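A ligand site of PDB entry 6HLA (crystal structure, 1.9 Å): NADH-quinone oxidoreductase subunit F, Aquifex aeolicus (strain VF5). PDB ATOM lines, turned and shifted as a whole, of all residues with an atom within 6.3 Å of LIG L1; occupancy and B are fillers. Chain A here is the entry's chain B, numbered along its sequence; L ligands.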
ATOM      1  N   ILE A 181     -17.649 -32.584 -26.581  1.00  0.00           N
ATOM      2  CA  ILE A 181     -17.274 -31.179 -26.544  1.00  0.00           C
ATOM      3  C   ILE A 181     -17.380 -30.485 -27.900  1.00  0.00           C
ATOM      4  O   ILE A 181     -17.525 -29.273 -27.947  1.00  0.00           O
ATOM      5  CB  ILE A 181     -15.861 -31.001 -25.908  1.00  0.00           C
ATOM      6  CG1 ILE A 181     -15.637 -29.572 -25.409  1.00  0.00           C
ATOM      7  CG2 ILE A 181     -14.723 -31.456 -26.841  1.00  0.00           C
ATOM      8  CD1 ILE A 181     -16.577 -29.120 -24.386  1.00  0.00           C
ATOM      9  N   GLU A 184     -20.184 -28.155 -28.489  1.00  0.00           N
ATOM     10  CA  GLU A 184     -20.013 -26.820 -27.945  1.00  0.00           C
ATOM     11  C   GLU A 184     -19.647 -26.034 -29.194  1.00  0.00           C
ATOM     12  O   GLU A 184     -18.775 -26.460 -29.966  1.00  0.00           O
ATOM     13  CB  GLU A 184     -18.895 -26.795 -26.877  1.00  0.00           C
ATOM     14  CG  GLU A 184     -18.976 -25.581 -25.967  1.00  0.00           C
ATOM     15  CD  GLU A 184     -18.378 -24.307 -26.511  1.00  0.00           C
ATOM     16  OE1 GLU A 184     -17.625 -24.366 -27.509  1.00  0.00           O
ATOM     17  OE2 GLU A 184     -18.650 -23.226 -25.918  1.00  0.00           O
ATOM     18  N   HIS A 198     -11.418 -27.840 -29.157  1.00  0.00           N
ATOM     19  CA  HIS A 198     -11.186 -27.051 -27.959  1.00  0.00           C
ATOM     20  C   HIS A 198     -12.032 -25.782 -27.950  1.00  0.00           C
ATOM     21  O   HIS A 198     -11.825 -24.919 -28.807  1.00  0.00           O
ATOM     22  CB  HIS A 198      -9.685 -26.725 -27.799  1.00  0.00           C
ATOM     23  CG  HIS A 198      -8.841 -27.890 -27.396  1.00  0.00           C
ATOM     24  ND1 HIS A 198      -7.456 -27.814 -27.418  1.00  0.00           N
ATOM     25  CD2 HIS A 198      -9.197 -29.105 -26.920  1.00  0.00           C
ATOM     26  CE1 HIS A 198      -7.028 -28.980 -26.968  1.00  0.00           C
ATOM     27  NE2 HIS A 198      -8.037 -29.799 -26.674  1.00  0.00           N
ATOM     28  N   PRO A 199     -12.972 -25.622 -26.967  1.00  0.00           N
ATOM     29  CA  PRO A 199     -13.760 -24.382 -26.893  1.00  0.00           C
ATOM     30  C   PRO A 199     -12.908 -23.123 -26.760  1.00  0.00           C
ATOM     31  O   PRO A 199     -11.839 -23.145 -26.119  1.00  0.00           O
ATOM     32  CB  PRO A 199     -14.614 -24.589 -25.656  1.00  0.00           C
ATOM     33  CG  PRO A 199     -14.748 -26.052 -25.559  1.00  0.00           C
ATOM     34  CD  PRO A 199     -13.392 -26.576 -25.920  1.00  0.00           C
ATOM     35  N   ARG A 200     -13.375 -22.021 -27.343  1.00  0.00           N
ATOM     36  CA  ARG A 200     -12.694 -20.713 -27.299  1.00  0.00           C
ATOM     37  C   ARG A 200     -13.345 -19.905 -26.199  1.00  0.00           C
ATOM     38  O   ARG A 200     -14.527 -20.099 -25.926  1.00  0.00           O
ATOM     39  CB  ARG A 200     -12.949 -19.942 -28.612  1.00  0.00           C
ATOM     40  CG  ARG A 200     -12.564 -20.684 -29.883  1.00  0.00           C
ATOM     41  CD  ARG A 200     -12.963 -19.864 -31.086  1.00  0.00           C
ATOM     42  NE  ARG A 200     -12.444 -20.437 -32.326  1.00  0.00           N
ATOM     43  CZ  ARG A 200     -12.657 -19.936 -33.539  1.00  0.00           C
ATOM     44  NH1 ARG A 200     -13.405 -18.851 -33.695  1.00  0.00           N
ATOM     45  NH2 ARG A 200     -12.129 -20.522 -34.603  1.00  0.00           N
ATOM     46  N   GLU A 345     -15.419 -36.661 -21.119  1.00  0.00           N
ATOM     47  CA  GLU A 345     -15.648 -35.602 -22.106  1.00  0.00           C
ATOM     48  C   GLU A 345     -14.946 -34.240 -21.887  1.00  0.00           C
ATOM     49  O   GLU A 345     -14.924 -33.427 -22.821  1.00  0.00           O
ATOM     50  CB  GLU A 345     -17.157 -35.389 -22.300  1.00  0.00           C
ATOM     51  CG  GLU A 345     -17.863 -36.654 -22.758  1.00  0.00           C
ATOM     52  CD  GLU A 345     -17.317 -37.372 -23.979  1.00  0.00           C
ATOM     53  OE1 GLU A 345     -16.689 -36.719 -24.850  1.00  0.00           O
ATOM     54  OE2 GLU A 345     -17.574 -38.584 -24.105  1.00  0.00           O
ATOM     55  N   THR A 346     -14.403 -33.978 -20.692  1.00  0.00           N
ATOM     56  CA  THR A 346     -13.668 -32.731 -20.452  1.00  0.00           C
ATOM     57  C   THR A 346     -12.530 -32.587 -21.460  1.00  0.00           C
ATOM     58  O   THR A 346     -11.837 -33.587 -21.707  1.00  0.00           O
ATOM     59  CB  THR A 346     -13.161 -32.631 -18.982  1.00  0.00           C
ATOM     60  OG1 THR A 346     -12.410 -31.426 -18.852  1.00  0.00           O
ATOM     61  CG2 THR A 346     -12.302 -33.828 -18.557  1.00  0.00           C
ATOM     62  N   CYS A 347     -12.363 -31.411 -22.078  1.00  0.00           N
ATOM     63  CA  CYS A 347     -11.253 -31.249 -23.037  1.00  0.00           C
ATOM     64  C   CYS A 347      -9.913 -30.987 -22.310  1.00  0.00           C
ATOM     65  O   CYS A 347      -8.839 -31.077 -22.918  1.00  0.00           O
ATOM     66  CB  CYS A 347     -11.568 -30.209 -24.107  1.00  0.00           C
ATOM     67  SG  CYS A 347     -11.321 -28.509 -23.577  1.00  0.00           S
ATOM     68  N   GLY A 348     -10.006 -30.684 -21.007  1.00  0.00           N
ATOM     69  CA  GLY A 348      -8.866 -30.475 -20.136  1.00  0.00           C
ATOM     70  C   GLY A 348      -8.082 -29.190 -20.306  1.00  0.00           C
ATOM     71  O   GLY A 348      -6.960 -29.102 -19.799  1.00  0.00           O
ATOM     72  N   GLN A 349      -8.669 -28.172 -20.994  1.00  0.00           N
ATOM     73  CA  GLN A 349      -8.031 -26.857 -21.197  1.00  0.00           C
ATOM     74  C   GLN A 349      -7.931 -26.095 -19.885  1.00  0.00           C
ATOM     75  O   GLN A 349      -6.941 -25.394 -19.635  1.00  0.00           O
ATOM     76  CB  GLN A 349      -8.889 -26.000 -22.138  1.00  0.00           C
ATOM     77  CG  GLN A 349      -8.548 -26.077 -23.611  1.00  0.00           C
ATOM     78  CD  GLN A 349      -9.248 -24.952 -24.329  1.00  0.00           C
ATOM     79  OE1 GLN A 349      -8.635 -23.951 -24.668  1.00  0.00           O
ATOM     80  NE2 GLN A 349     -10.559 -25.087 -24.541  1.00  0.00           N
ATOM     81  N   CYS A 350      -9.009 -26.170 -19.111  1.00  0.00           N
ATOM     82  CA  CYS A 350      -9.197 -25.507 -17.827  1.00  0.00           C
ATOM     83  C   CYS A 350      -8.886 -26.516 -16.744  1.00  0.00           C
ATOM     84  O   CYS A 350      -9.435 -27.606 -16.752  1.00  0.00           O
ATOM     85  CB  CYS A 350     -10.621 -24.979 -17.714  1.00  0.00           C
ATOM     86  SG  CYS A 350     -11.261 -24.234 -19.249  1.00  0.00           S
ATOM     87  N   THR A 351      -7.952 -26.152 -15.843  1.00  0.00           N
ATOM     88  CA  THR A 351      -7.477 -26.998 -14.732  1.00  0.00           C
ATOM     89  C   THR A 351      -8.628 -27.494 -13.832  1.00  0.00           C
ATOM     90  O   THR A 351      -8.712 -28.709 -13.683  1.00  0.00           O
ATOM     91  CB  THR A 351      -6.331 -26.321 -13.961  1.00  0.00           C
ATOM     92  OG1 THR A 351      -5.222 -26.128 -14.842  1.00  0.00           O
ATOM     93  CG2 THR A 351      -5.859 -27.133 -12.756  1.00  0.00           C
ATOM     94  N   CYS A 353     -11.771 -27.955 -14.388  1.00  0.00           N
ATOM     95  CA  CYS A 353     -12.613 -28.874 -15.163  1.00  0.00           C
ATOM     96  C   CYS A 353     -11.855 -30.181 -15.398  1.00  0.00           C
ATOM     97  O   CYS A 353     -12.388 -31.271 -15.091  1.00  0.00           O
ATOM     98  CB  CYS A 353     -13.058 -28.239 -16.490  1.00  0.00           C
ATOM     99  SG  CYS A 353     -14.112 -29.304 -17.500  1.00  0.00           S
ATOM    100  N   ARG A 354     -10.604 -30.073 -15.890  1.00  0.00           N
ATOM    101  CA  ARG A 354      -9.727 -31.219 -16.140  1.00  0.00           C
ATOM    102  C   ARG A 354      -9.610 -32.141 -14.890  1.00  0.00           C
ATOM    103  O   ARG A 354      -9.996 -33.315 -14.956  1.00  0.00           O
ATOM    104  CB  ARG A 354      -8.348 -30.742 -16.598  1.00  0.00           C
ATOM    105  CG  ARG A 354      -7.311 -31.856 -16.834  1.00  0.00           C
ATOM    106  CD  ARG A 354      -5.981 -31.328 -17.358  1.00  0.00           C
ATOM    107  NE  ARG A 354      -5.184 -30.632 -16.330  1.00  0.00           N
ATOM    108  CZ  ARG A 354      -4.994 -29.311 -16.296  1.00  0.00           C
ATOM    109  NH1 ARG A 354      -5.536 -28.528 -17.232  1.00  0.00           N
ATOM    110  NH2 ARG A 354      -4.235 -28.774 -15.360  1.00  0.00           N
ATOM    111  N   CYS A 357     -13.427 -33.085 -13.164  1.00  0.00           N
ATOM    112  CA  CYS A 357     -14.196 -34.132 -13.833  1.00  0.00           C
ATOM    113  C   CYS A 357     -13.616 -35.484 -13.551  1.00  0.00           C
ATOM    114  O   CYS A 357     -14.372 -36.409 -13.228  1.00  0.00           O
ATOM    115  CB  CYS A 357     -14.317 -33.873 -15.321  1.00  0.00           C
ATOM    116  SG  CYS A 357     -15.450 -32.514 -15.713  1.00  0.00           S
ATOM    117  N   ILE A 387     -15.684 -27.506  -9.981  1.00  0.00           N
ATOM    118  CA  ILE A 387     -15.322 -27.883 -11.352  1.00  0.00           C
ATOM    119  C   ILE A 387     -15.414 -26.605 -12.192  1.00  0.00           C
ATOM    120  O   ILE A 387     -14.584 -26.352 -13.057  1.00  0.00           O
ATOM    121  CB  ILE A 387     -16.200 -29.052 -11.928  1.00  0.00           C
ATOM    122  CG1 ILE A 387     -16.206 -30.283 -10.970  1.00  0.00           C
ATOM    123  CG2 ILE A 387     -15.768 -29.456 -13.333  1.00  0.00           C
ATOM    124  CD1 ILE A 387     -17.300 -31.360 -11.217  1.00  0.00           C
ATOM    125  N   THR A 390     -12.859 -20.870 -13.390  1.00  0.00           N
ATOM    126  CA  THR A 390     -12.055 -20.519 -14.583  1.00  0.00           C
ATOM    127  C   THR A 390     -12.517 -21.189 -15.893  1.00  0.00           C
ATOM    128  O   THR A 390     -11.924 -20.897 -16.924  1.00  0.00           O
ATOM    129  CB  THR A 390     -10.509 -20.746 -14.351  1.00  0.00           C
ATOM    130  OG1 THR A 390     -10.193 -22.135 -14.484  1.00  0.00           O
ATOM    131  CG2 THR A 390     -10.008 -20.211 -13.006  1.00  0.00           C
ATOM    132  N   SER A 391     -13.585 -22.043 -15.882  1.00  0.00           N
ATOM    133  CA  SER A 391     -14.085 -22.739 -17.084  1.00  0.00           C
ATOM    134  C   SER A 391     -14.428 -21.774 -18.216  1.00  0.00           C
ATOM    135  O   SER A 391     -14.987 -20.716 -17.959  1.00  0.00           O
ATOM    136  CB  SER A 391     -15.308 -23.597 -16.765  1.00  0.00           C
ATOM    137  OG  SER A 391     -16.346 -22.845 -16.163  1.00  0.00           O
ATOM    138  N   ILE A 392     -14.076 -22.129 -19.461  1.00  0.00           N
ATOM    139  CA  ILE A 392     -14.383 -21.262 -20.596  1.00  0.00           C
ATOM    140  C   ILE A 392     -15.531 -21.823 -21.464  1.00  0.00           C
ATOM    141  O   ILE A 392     -15.823 -21.237 -22.511  1.00  0.00           O
ATOM    142  CB  ILE A 392     -13.140 -20.829 -21.450  1.00  0.00           C
ATOM    143  CG1 ILE A 392     -12.327 -22.039 -21.969  1.00  0.00           C
ATOM    144  CG2 ILE A 392     -12.282 -19.848 -20.647  1.00  0.00           C
ATOM    145  CD1 ILE A 392     -11.283 -21.722 -23.066  1.00  0.00           C
ATOM    146  N   CYS A 393     -16.222 -22.890 -21.021  1.00  0.00           N
ATOM    147  CA  CYS A 393     -17.405 -23.439 -21.711  1.00  0.00           C
ATOM    148  C   CYS A 393     -18.383 -24.047 -20.708  1.00  0.00           C
ATOM    149  O   CYS A 393     -18.056 -24.189 -19.524  1.00  0.00           O
ATOM    150  CB  CYS A 393     -17.046 -24.390 -22.858  1.00  0.00           C
ATOM    151  SG  CYS A 393     -17.017 -26.156 -22.460  1.00  0.00           S
ATOM    152  N   GLY A 394     -19.601 -24.326 -21.172  1.00  0.00           N
ATOM    153  CA  GLY A 394     -20.683 -24.837 -20.325  1.00  0.00           C
ATOM    154  C   GLY A 394     -20.440 -26.179 -19.651  1.00  0.00           C
ATOM    155  O   GLY A 394     -21.091 -26.453 -18.648  1.00  0.00           O
ATOM    156  N   LEU A 395     -19.534 -27.023 -20.189  1.00  0.00           N
ATOM    157  CA  LEU A 395     -19.210 -28.352 -19.642  1.00  0.00           C
ATOM    158  C   LEU A 395     -18.671 -28.273 -18.191  1.00  0.00           C
ATOM    159  O   LEU A 395     -19.191 -28.979 -17.314  1.00  0.00           O
ATOM    160  CB  LEU A 395     -18.245 -29.148 -20.573  1.00  0.00           C
ATOM    161  CG  LEU A 395     -18.109 -30.656 -20.267  1.00  0.00           C
ATOM    162  CD1 LEU A 395     -17.686 -31.409 -21.483  1.00  0.00           C
ATOM    163  CD2 LEU A 395     -17.073 -30.923 -19.113  1.00  0.00           C
ATOM    164  N   GLY A 396     -17.676 -27.422 -17.954  1.00  0.00           N
ATOM    165  CA  GLY A 396     -17.098 -27.225 -16.621  1.00  0.00           C
ATOM    166  C   GLY A 396     -18.112 -26.580 -15.702  1.00  0.00           C
ATOM    167  O   GLY A 396     -18.173 -26.897 -14.511  1.00  0.00           O
ATOM    168  N   ALA A 397     -18.974 -25.703 -16.273  1.00  0.00           N
ATOM    169  CA  ALA A 397     -20.006 -25.008 -15.512  1.00  0.00           C
ATOM    170  C   ALA A 397     -21.101 -25.933 -14.975  1.00  0.00           C
ATOM    171  O   ALA A 397     -21.726 -25.615 -13.963  1.00  0.00           O
ATOM    172  CB  ALA A 397     -20.625 -23.882 -16.337  1.00  0.00           C
HETATM  173 FE1  LIG L   1     -12.665 -27.852 -21.921  1.00  0.00          FE
HETATM  174 FE2  LIG L   1     -13.856 -28.149 -19.458  1.00  0.00          FE
HETATM  175 FE3  LIG L   1     -15.019 -26.537 -21.357  1.00  0.00          FE
HETATM  176 FE4  LIG L   1     -12.666 -25.780 -20.103  1.00  0.00          FE
HETATM  177  S1  LIG L   1     -14.741 -26.068 -19.127  1.00  0.00           S
HETATM  178  S2  LIG L   1     -13.131 -25.605 -22.357  1.00  0.00           S
HETATM  179  S3  LIG L   1     -11.613 -27.814 -19.879  1.00  0.00           S
HETATM  180  S4  LIG L   1     -14.708 -28.801 -21.484  1.00  0.00           S
HETATM  181  N1  LG2 L   2     -25.948 -27.712 -29.109  1.00  0.00           N
HETATM  182  C1  LG2 L   2     -26.399 -28.534 -30.107  1.00  0.00           C
HETATM  183  O1  LG2 L   2     -27.174 -28.124 -30.971  1.00  0.00           O
HETATM  184  N2  LG2 L   2     -25.908 -29.836 -30.208  1.00  0.00           N
HETATM  185  C2  LG2 L   2     -24.933 -30.405 -29.398  1.00  0.00           C
HETATM  186  O2  LG2 L   2     -24.582 -31.568 -29.586  1.00  0.00           O
HETATM  187  C3  LG2 L   2     -24.426 -29.501 -28.361  1.00  0.00           C
HETATM  188  N3  LG2 L   2     -23.433 -29.918 -27.615  1.00  0.00           N
HETATM  189  C4  LG2 L   2     -22.901 -29.031 -26.674  1.00  0.00           C
HETATM  190  C5  LG2 L   2     -21.875 -29.475 -25.830  1.00  0.00           C
HETATM  191  C6  LG2 L   2     -21.386 -28.668 -24.811  1.00  0.00           C
HETATM  192  C7  LG2 L   2     -20.303 -29.198 -23.902  1.00  0.00           C
HETATM  193  C8  LG2 L   2     -21.910 -27.375 -24.646  1.00  0.00           C
HETATM  194  C9  LG2 L   2     -21.422 -26.463 -23.535  1.00  0.00           C
HETATM  195  C10 LG2 L   2     -22.905 -26.915 -25.502  1.00  0.00           C
HETATM  196  C11 LG2 L   2     -23.409 -27.736 -26.514  1.00  0.00           C
HETATM  197  N4  LG2 L   2     -24.474 -27.312 -27.369  1.00  0.00           N
HETATM  198  C12 LG2 L   2     -25.010 -28.169 -28.296  1.00  0.00           C
HETATM  199  C13 LG2 L   2     -24.931 -25.917 -27.353  1.00  0.00           C
HETATM  200  C14 LG2 L   2     -24.226 -25.055 -28.399  1.00  0.00           C
HETATM  201  O3  LG2 L   2     -22.976 -24.586 -27.877  1.00  0.00           O
HETATM  202  C15 LG2 L   2     -25.117 -23.902 -28.855  1.00  0.00           C
HETATM  203  O4  LG2 L   2     -25.770 -23.307 -27.728  1.00  0.00           O
HETATM  204  C16 LG2 L   2     -26.196 -24.255 -29.886  1.00  0.00           C
HETATM  205  O5  LG2 L   2     -25.730 -25.175 -30.881  1.00  0.00           O
HETATM  206  C17 LG2 L   2     -26.770 -23.022 -30.531  1.00  0.00           C
HETATM  207  O6  LG2 L   2     -27.953 -23.404 -31.265  1.00  0.00           O
HETATM  208  P1  LG2 L   2     -29.413 -23.092 -30.794  1.00  0.00           P
HETATM  209  O7  LG2 L   2     -29.788 -23.944 -29.666  1.00  0.00           O
HETATM  210  O8  LG2 L   2     -29.419 -21.605 -30.376  1.00  0.00           O
HETATM  211  O9  LG2 L   2     -30.310 -23.289 -32.041  1.00  0.00           O
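A sulfur (S1) of LIG L1 lies close to the backbone NH of Gly 396 (3.4 Å).
The side-chain sulfur of Cys 353 is bound to an iron atom (FE2) of LIG L1 (2.3 Å).
A sulfur (S3) of LIG L1 lies close to the backbone NH (N) of Gly 348, 3.5 Å away.
A sulfur (S2) of LIG L1 lies close to the side-chain amide nitrogen of Gln 349 (3.4 Å).
The side-chain sulfur (SG) of Cys 350 is bound to an iron atom (FE4) of LIG L1 (2.3 Å).
N of Cys 350 sits close to S3 of LIG L1 (3.2 Å).
N of Gln 349 lies close to S3 of LIG L1.
SG of Cys 347 is bound to FE1 of LIG L1.
A sulfur (S4) of LIG L1 sits close to the backbone NH (N) of Cys 347 (3.6 Å).
The side-chain sulfur of Cys 393 is bound to an iron atom (FE3) of LIG L1, 2.3 Å away.
Residues that only touch LIG L1: Ile 181, Pro 199, Thr 346, Ser 391, Ile 392 and Leu 395.
The backbone carbonyl oxygen (O) of Gly 348 sits at hydrogen-bond distance from the guanidinium group (NH1) of Arg 354, 3.0 Å away.
The side-chain sulfur of Cys 350 lies close to the backbone NH of Ile 392.
The backbone carbonyl oxygen (O) of Cys 353 sits close to the side-chain sulfur (SG) of Cys 357, 3.4 Å away.
SG of Cys 393 sits close to N of Leu 395.
SG of Cys 347 sits close to NE2 of Gln 349 (3.6 Å).
The side-chain sulfur of Cys 353 sits close to the side-chain hydroxyl of Thr 346 (3.0 Å).
N of Gly 348 lies close to OG1 of Thr 346, 3.3 Å away.
O of Pro 199 lies within hydrogen-bond range of NE2 of Gln 349, 2.8 Å away.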
